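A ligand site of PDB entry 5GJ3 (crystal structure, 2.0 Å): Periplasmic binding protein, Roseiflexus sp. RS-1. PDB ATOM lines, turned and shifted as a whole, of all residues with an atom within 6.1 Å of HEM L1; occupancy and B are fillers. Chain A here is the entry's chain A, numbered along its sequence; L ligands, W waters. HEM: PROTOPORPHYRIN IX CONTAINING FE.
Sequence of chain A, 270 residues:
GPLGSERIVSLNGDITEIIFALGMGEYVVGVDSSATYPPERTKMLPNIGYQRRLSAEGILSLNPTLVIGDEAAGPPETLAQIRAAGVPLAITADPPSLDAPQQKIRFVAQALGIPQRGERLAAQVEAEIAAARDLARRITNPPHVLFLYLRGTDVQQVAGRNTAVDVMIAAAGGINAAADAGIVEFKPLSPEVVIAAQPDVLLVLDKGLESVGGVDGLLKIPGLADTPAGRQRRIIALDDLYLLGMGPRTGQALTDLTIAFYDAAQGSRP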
ATOM      1  N   SER A  33      22.887  -6.525  -2.122  1.00  0.00           N
ATOM      2  CA  SER A  33      22.757  -7.098  -3.515  1.00  0.00           C
ATOM      3  C   SER A  33      21.497  -6.736  -4.273  1.00  0.00           C
ATOM      4  O   SER A  33      21.508  -6.664  -5.490  1.00  0.00           O
ATOM      5  CB  SER A  33      22.736  -8.631  -3.455  1.00  0.00           C
ATOM      6  OG  SER A  33      23.979  -9.081  -3.021  1.00  0.00           O
ATOM      7  N   SER A  34      20.377  -6.583  -3.567  1.00  0.00           N
ATOM      8  CA  SER A  34      19.114  -6.282  -4.263  1.00  0.00           C
ATOM      9  C   SER A  34      18.966  -4.783  -4.578  1.00  0.00           C
ATOM     10  O   SER A  34      17.940  -4.355  -5.117  1.00  0.00           O
ATOM     11  CB  SER A  34      17.898  -6.769  -3.446  1.00  0.00           C
ATOM     12  OG  SER A  34      17.712  -5.895  -2.326  1.00  0.00           O
ATOM     13  N   THR A  36      19.339  -2.240  -6.765  1.00  0.00           N
ATOM     14  CA  THR A  36      19.674  -2.028  -8.206  1.00  0.00           C
ATOM     15  C   THR A  36      19.104  -0.678  -8.726  1.00  0.00           C
ATOM     16  O   THR A  36      19.128  -0.458  -9.936  1.00  0.00           O
ATOM     17  CB  THR A  36      19.055  -3.158  -9.049  1.00  0.00           C
ATOM     18  OG1 THR A  36      17.703  -3.283  -8.650  1.00  0.00           O
ATOM     19  CG2 THR A  36      19.737  -4.488  -8.856  1.00  0.00           C
ATOM     20  N   TYR A  50      23.529 -10.117   0.511  1.00  0.00           N
ATOM     21  CA  TYR A  50      22.098 -10.072   0.141  1.00  0.00           C
ATOM     22  C   TYR A  50      21.225  -9.650   1.390  1.00  0.00           C
ATOM     23  O   TYR A  50      21.552 -10.021   2.503  1.00  0.00           O
ATOM     24  CB  TYR A  50      21.634 -11.418  -0.475  1.00  0.00           C
ATOM     25  CG  TYR A  50      20.147 -11.448  -0.799  1.00  0.00           C
ATOM     26  CD1 TYR A  50      19.588 -10.527  -1.691  1.00  0.00           C
ATOM     27  CD2 TYR A  50      19.303 -12.349  -0.163  1.00  0.00           C
ATOM     28  CE1 TYR A  50      18.208 -10.494  -1.932  1.00  0.00           C
ATOM     29  CE2 TYR A  50      17.903 -12.358  -0.407  1.00  0.00           C
ATOM     30  CZ  TYR A  50      17.377 -11.430  -1.290  1.00  0.00           C
ATOM     31  OH  TYR A  50      16.001 -11.418  -1.521  1.00  0.00           O
ATOM     32  N   GLN A  51      20.158  -8.901   1.173  1.00  0.00           N
ATOM     33  CA  GLN A  51      19.259  -8.412   2.279  1.00  0.00           C
ATOM     34  C   GLN A  51      18.876  -9.425   3.367  1.00  0.00           C
ATOM     35  O   GLN A  51      18.753  -9.045   4.523  1.00  0.00           O
ATOM     36  CB  GLN A  51      17.999  -7.713   1.727  1.00  0.00           C
ATOM     37  CG  GLN A  51      16.992  -8.653   1.016  1.00  0.00           C
ATOM     38  CD  GLN A  51      15.948  -7.880   0.224  1.00  0.00           C
ATOM     39  OE1 GLN A  51      15.593  -6.728   0.577  1.00  0.00           O
ATOM     40  NE2 GLN A  51      15.454  -8.492  -0.850  1.00  0.00           N
ATOM     41  N   ARG A  52      18.716 -10.705   2.994  1.00  0.00           N
ATOM     42  CA  ARG A  52      18.348 -11.768   3.962  1.00  0.00           C
ATOM     43  C   ARG A  52      19.557 -12.560   4.424  1.00  0.00           C
ATOM     44  O   ARG A  52      19.436 -13.467   5.225  1.00  0.00           O
ATOM     45  CB  ARG A  52      17.389 -12.780   3.297  1.00  0.00           C
ATOM     46  CG  ARG A  52      16.069 -12.146   2.841  1.00  0.00           C
ATOM     47  CD  ARG A  52      15.049 -13.235   2.487  1.00  0.00           C
ATOM     48  NE  ARG A  52      13.665 -12.756   2.589  1.00  0.00           N
ATOM     49  CZ  ARG A  52      13.118 -11.806   1.816  1.00  0.00           C
ATOM     50  NH1 ARG A  52      13.815 -11.171   0.881  1.00  0.00           N
ATOM     51  NH2 ARG A  52      11.845 -11.480   1.981  1.00  0.00           N
ATOM     52  N   ARG A  53      20.739 -12.199   3.931  1.00  0.00           N
ATOM     53  CA  ARG A  53      21.945 -12.936   4.290  1.00  0.00           C
ATOM     54  C   ARG A  53      23.085 -11.905   4.497  1.00  0.00           C
ATOM     55  O   ARG A  53      24.193 -12.000   3.908  1.00  0.00           O
ATOM     56  CB  ARG A  53      22.248 -14.017   3.171  1.00  0.00           C
ATOM     57  CG  ARG A  53      22.901 -15.321   3.694  1.00  0.00           C
ATOM     58  CD  ARG A  53      23.067 -16.451   2.650  1.00  0.00           C
ATOM     59  NE  ARG A  53      24.021 -16.047   1.633  1.00  0.00           N
ATOM     60  CZ  ARG A  53      23.689 -15.516   0.466  1.00  0.00           C
ATOM     61  NH1 ARG A  53      22.397 -15.309   0.190  1.00  0.00           N
ATOM     62  NH2 ARG A  53      24.629 -15.137  -0.418  1.00  0.00           N
ATOM     63  N   TYR A 149       7.570 -16.948 -11.160  1.00  0.00           N
ATOM     64  CA  TYR A 149       8.929 -16.778 -10.717  1.00  0.00           C
ATOM     65  C   TYR A 149       9.756 -17.892 -11.418  1.00  0.00           C
ATOM     66  O   TYR A 149       9.433 -19.077 -11.276  1.00  0.00           O
ATOM     67  CB  TYR A 149       8.976 -16.912  -9.203  1.00  0.00           C
ATOM     68  CG  TYR A 149      10.391 -16.900  -8.695  1.00  0.00           C
ATOM     69  CD1 TYR A 149      11.081 -15.694  -8.527  1.00  0.00           C
ATOM     70  CD2 TYR A 149      11.080 -18.115  -8.423  1.00  0.00           C
ATOM     71  CE1 TYR A 149      12.417 -15.661  -8.076  1.00  0.00           C
ATOM     72  CE2 TYR A 149      12.423 -18.102  -7.984  1.00  0.00           C
ATOM     73  CZ  TYR A 149      13.090 -16.882  -7.779  1.00  0.00           C
ATOM     74  OH  TYR A 149      14.408 -16.832  -7.325  1.00  0.00           O
ATOM     75  N   PHE A 186       4.076 -18.673  -2.605  1.00  0.00           N
ATOM     76  CA  PHE A 186       4.734 -19.325  -3.751  1.00  0.00           C
ATOM     77  C   PHE A 186       4.529 -20.824  -3.811  1.00  0.00           C
ATOM     78  O   PHE A 186       4.771 -21.537  -2.826  1.00  0.00           O
ATOM     79  CB  PHE A 186       6.233 -19.011  -3.770  1.00  0.00           C
ATOM     80  CG  PHE A 186       6.553 -17.616  -4.200  1.00  0.00           C
ATOM     81  CD1 PHE A 186       6.285 -16.542  -3.343  1.00  0.00           C
ATOM     82  CD2 PHE A 186       7.079 -17.359  -5.447  1.00  0.00           C
ATOM     83  CE1 PHE A 186       6.558 -15.242  -3.740  1.00  0.00           C
ATOM     84  CE2 PHE A 186       7.351 -16.064  -5.852  1.00  0.00           C
ATOM     85  CZ  PHE A 186       7.091 -15.005  -4.999  1.00  0.00           C
ATOM     86  N   ASP A 240      12.468  -6.748 -11.335  1.00  0.00           N
ATOM     87  CA  ASP A 240      11.994  -7.131 -10.005  1.00  0.00           C
ATOM     88  C   ASP A 240      11.784  -6.013  -8.968  1.00  0.00           C
ATOM     89  O   ASP A 240      10.739  -5.967  -8.320  1.00  0.00           O
ATOM     90  CB  ASP A 240      12.844  -8.229  -9.352  1.00  0.00           C
ATOM     91  CG  ASP A 240      14.364  -8.002  -9.519  1.00  0.00           C
ATOM     92  OD1 ASP A 240      14.800  -6.844  -9.623  1.00  0.00           O
ATOM     93  OD2 ASP A 240      15.113  -9.011  -9.553  1.00  0.00           O
ATOM     94  N   LEU A 241      12.771  -5.120  -8.788  1.00  0.00           N
ATOM     95  CA  LEU A 241      12.593  -4.064  -7.787  1.00  0.00           C
ATOM     96  C   LEU A 241      11.403  -3.117  -8.200  1.00  0.00           C
ATOM     97  O   LEU A 241      10.630  -2.659  -7.375  1.00  0.00           O
ATOM     98  CB  LEU A 241      13.915  -3.273  -7.583  1.00  0.00           C
ATOM     99  CG  LEU A 241      14.009  -2.254  -6.436  1.00  0.00           C
ATOM    100  CD1 LEU A 241      13.583  -2.805  -5.070  1.00  0.00           C
ATOM    101  CD2 LEU A 241      15.423  -1.676  -6.362  1.00  0.00           C
ATOM    102  N   LEU A 244       7.989  -5.237  -7.732  1.00  0.00           N
ATOM    103  CA  LEU A 244       7.734  -5.848  -6.432  1.00  0.00           C
ATOM    104  C   LEU A 244       8.244  -5.072  -5.192  1.00  0.00           C
ATOM    105  O   LEU A 244       7.869  -5.414  -4.056  1.00  0.00           O
ATOM    106  CB  LEU A 244       8.327  -7.264  -6.411  1.00  0.00           C
ATOM    107  CG  LEU A 244       7.755  -8.227  -7.454  1.00  0.00           C
ATOM    108  CD1 LEU A 244       8.552  -9.512  -7.335  1.00  0.00           C
ATOM    109  CD2 LEU A 244       6.267  -8.509  -7.161  1.00  0.00           C
ATOM    110  N   GLY A 245       9.064  -4.031  -5.419  1.00  0.00           N
ATOM    111  CA  GLY A 245       9.585  -3.169  -4.330  1.00  0.00           C
ATOM    112  C   GLY A 245       8.611  -2.378  -3.435  1.00  0.00           C
ATOM    113  O   GLY A 245       8.951  -2.060  -2.282  1.00  0.00           O
HETATM  114  CHA HEM L   1      17.795 -14.289  -3.380  1.00  0.00           C
HETATM  115  CHB HEM L   1      16.528  -9.918  -5.114  1.00  0.00           C
HETATM  116  CHC HEM L   1      12.281 -10.554  -2.759  1.00  0.00           C
HETATM  117  CHD HEM L   1      13.845 -14.633  -0.646  1.00  0.00           C
HETATM  118  C1A HEM L   1      17.782 -13.090  -4.058  1.00  0.00           C
HETATM  119  C2A HEM L   1      18.888 -12.627  -4.800  1.00  0.00           C
HETATM  120  C3A HEM L   1      18.587 -11.388  -5.283  1.00  0.00           C
HETATM  121  C4A HEM L   1      17.247 -11.099  -4.847  1.00  0.00           C
HETATM  122  CMA HEM L   1      19.491 -10.492  -6.136  1.00  0.00           C
HETATM  123  CAA HEM L   1      20.190 -13.393  -4.957  1.00  0.00           C
HETATM  124  CBA HEM L   1      20.952 -13.241  -3.614  1.00  0.00           C
HETATM  125  CGA HEM L   1      22.020 -14.285  -3.391  1.00  0.00           C
HETATM  126  O1A HEM L   1      22.014 -15.316  -4.065  1.00  0.00           O
HETATM  127  O2A HEM L   1      22.901 -14.164  -2.506  1.00  0.00           O
HETATM  128  C1B HEM L   1      15.210  -9.732  -4.640  1.00  0.00           C
HETATM  129  C2B HEM L   1      14.362  -8.615  -4.981  1.00  0.00           C
HETATM  130  C3B HEM L   1      13.157  -8.812  -4.345  1.00  0.00           C
HETATM  131  C4B HEM L   1      13.313 -10.057  -3.575  1.00  0.00           C
HETATM  132  CMB HEM L   1      14.700  -7.483  -5.916  1.00  0.00           C
HETATM  133  CAB HEM L   1      11.921  -7.983  -4.327  1.00  0.00           C
HETATM  134  CBB HEM L   1      11.983  -6.658  -4.586  1.00  0.00           C
HETATM  135  C1C HEM L   1      12.286 -11.717  -2.033  1.00  0.00           C
HETATM  136  C2C HEM L   1      11.177 -12.286  -1.373  1.00  0.00           C
HETATM  137  C3C HEM L   1      11.629 -13.465  -0.760  1.00  0.00           C
HETATM  138  C4C HEM L   1      13.021 -13.605  -1.087  1.00  0.00           C
HETATM  139  CMC HEM L   1       9.778 -11.662  -1.362  1.00  0.00           C
HETATM  140  CAC HEM L   1      10.856 -14.432   0.075  1.00  0.00           C
HETATM  141  CBC HEM L   1       9.545 -14.328   0.279  1.00  0.00           C
HETATM  142  C1D HEM L   1      15.058 -14.847  -1.298  1.00  0.00           C
HETATM  143  C2D HEM L   1      15.857 -16.057  -0.992  1.00  0.00           C
HETATM  144  C3D HEM L   1      16.950 -15.963  -1.749  1.00  0.00           C
HETATM  145  C4D HEM L   1      16.816 -14.705  -2.502  1.00  0.00           C
HETATM  146  CMD HEM L   1      15.486 -17.183  -0.039  1.00  0.00           C
HETATM  147  CAD HEM L   1      18.110 -16.952  -1.792  1.00  0.00           C
HETATM  148  CBD HEM L   1      19.264 -16.249  -0.976  1.00  0.00           C
HETATM  149  CGD HEM L   1      19.266 -16.488   0.530  1.00  0.00           C
HETATM  150  O1D HEM L   1      18.701 -17.484   1.019  1.00  0.00           O
HETATM  151  O2D HEM L   1      19.875 -15.726   1.337  1.00  0.00           O
HETATM  152  NA  HEM L   1      16.833 -12.135  -4.025  1.00  0.00           N
HETATM  153  NB  HEM L   1      14.562 -10.505  -3.772  1.00  0.00           N
HETATM  154  NC  HEM L   1      13.388 -12.510  -1.839  1.00  0.00           N
HETATM  155  ND  HEM L   1      15.692 -14.011  -2.185  1.00  0.00           N
HETATM  156 FE   HEM L   1      15.165 -12.308  -2.926  1.00  0.00          FE
HETATM  157  CHA HEM L   2      18.339 -16.181  -7.096  1.00  0.00           C
HETATM  158  CHB HEM L   2      14.922 -12.718  -7.242  1.00  0.00           C
HETATM  159  CHC HEM L   2      12.012 -15.295  -4.254  1.00  0.00           C
HETATM  160  CHD HEM L   2      15.561 -18.622  -3.926  1.00  0.00           C
HETATM  161  C1A HEM L   2      17.654 -15.023  -7.341  1.00  0.00           C
HETATM  162  C2A HEM L   2      18.204 -13.917  -8.048  1.00  0.00           C
HETATM  163  C3A HEM L   2      17.247 -12.948  -8.089  1.00  0.00           C
HETATM  164  C4A HEM L   2      16.108 -13.447  -7.397  1.00  0.00           C
HETATM  165  CMA HEM L   2      17.335 -11.584  -8.764  1.00  0.00           C
HETATM  166  CAA HEM L   2      19.612 -13.843  -8.643  1.00  0.00           C
HETATM  167  CBA HEM L   2      19.637 -13.981 -10.181  1.00  0.00           C
HETATM  168  CGA HEM L   2      19.383 -15.381 -10.677  1.00  0.00           C
HETATM  169  O1A HEM L   2      18.865 -16.265  -9.963  1.00  0.00           O
HETATM  170  O2A HEM L   2      19.667 -15.701 -11.846  1.00  0.00           O
HETATM  171  C1B HEM L   2      13.851 -13.127  -6.436  1.00  0.00           C
HETATM  172  C2B HEM L   2      12.676 -12.324  -6.238  1.00  0.00           C
HETATM  173  C3B HEM L   2      11.856 -13.010  -5.394  1.00  0.00           C
HETATM  174  C4B HEM L   2      12.561 -14.295  -5.066  1.00  0.00           C
HETATM  175  CMB HEM L   2      12.423 -10.971  -6.862  1.00  0.00           C
HETATM  176  CAB HEM L   2      10.531 -12.617  -4.896  1.00  0.00           C
HETATM  177  CBB HEM L   2       9.484 -12.874  -5.643  1.00  0.00           C
HETATM  178  C1C HEM L   2      12.744 -16.434  -3.863  1.00  0.00           C
HETATM  179  C2C HEM L   2      12.347 -17.331  -2.852  1.00  0.00           C
HETATM  180  C3C HEM L   2      13.367 -18.303  -2.753  1.00  0.00           C
HETATM  181  C4C HEM L   2      14.363 -17.956  -3.719  1.00  0.00           C
HETATM  182  CMC HEM L   2      11.049 -17.231  -2.082  1.00  0.00           C
HETATM  183  CAC HEM L   2      13.485 -19.512  -1.879  1.00  0.00           C
HETATM  184  CBC HEM L   2      12.462 -20.094  -1.266  1.00  0.00           C
HETATM  185  C1D HEM L   2      16.585 -18.159  -4.748  1.00  0.00           C
HETATM  186  C2D HEM L   2      17.864 -18.916  -4.876  1.00  0.00           C
HETATM  187  C3D HEM L   2      18.638 -18.241  -5.772  1.00  0.00           C
HETATM  188  C4D HEM L   2      17.819 -17.082  -6.176  1.00  0.00           C
HETATM  189  CMD HEM L   2      18.182 -20.180  -4.115  1.00  0.00           C
HETATM  190  CAD HEM L   2      20.045 -18.580  -6.249  1.00  0.00           C
HETATM  191  CBD HEM L   2      21.214 -17.978  -5.418  1.00  0.00           C
HETATM  192  CGD HEM L   2      22.546 -18.236  -6.112  1.00  0.00           C
HETATM  193  O1D HEM L   2      23.649 -17.741  -5.730  1.00  0.00           O
HETATM  194  O2D HEM L   2      22.609 -18.990  -7.104  1.00  0.00           O
HETATM  195  NA  HEM L   2      16.339 -14.733  -6.938  1.00  0.00           N
HETATM  196  NB  HEM L   2      13.703 -14.278  -5.785  1.00  0.00           N
HETATM  197  NC  HEM L   2      13.969 -16.817  -4.379  1.00  0.00           N
HETATM  198  ND  HEM L   2      16.568 -17.131  -5.622  1.00  0.00           N
HETATM  199 FE   HEM L   2      15.179 -15.796  -5.725  1.00  0.00          FE
HETATM  200  O   HOH W   1      24.088 -11.875  -3.080  1.00  0.00           O
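The side-chain hydroxyl of Tyr 50 is bound to an iron atom (FE) of HEM L1, at 1.9 Å. NH1 of Arg 53 is in salt-bridge range of O2D of HEM L1, 2.8 Å away. FE of HEM L2 is bound by OH of Tyr 149 (2.1 Å).
The side-chain hydroxyl of Tyr 50 sits close to the side-chain amide nitrogen of Gln 51 (3.1 Å). OH of Tyr 50 lies close to NH1 of Arg 52, 3.3 Å away.
NH1 of Arg 52 sits close to NC of HEM L1 (3.1 Å). Merely in contact with HEM L1: Ser 34, Gln 51 and Asp 240. Hydrophobic or aromatic side chains within 4 Å of HEM L1: Tyr 50.
Water W1 bridges an oxygen (O2A) of HEM L1 and the side-chain hydroxyl (OG) of Ser 33.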
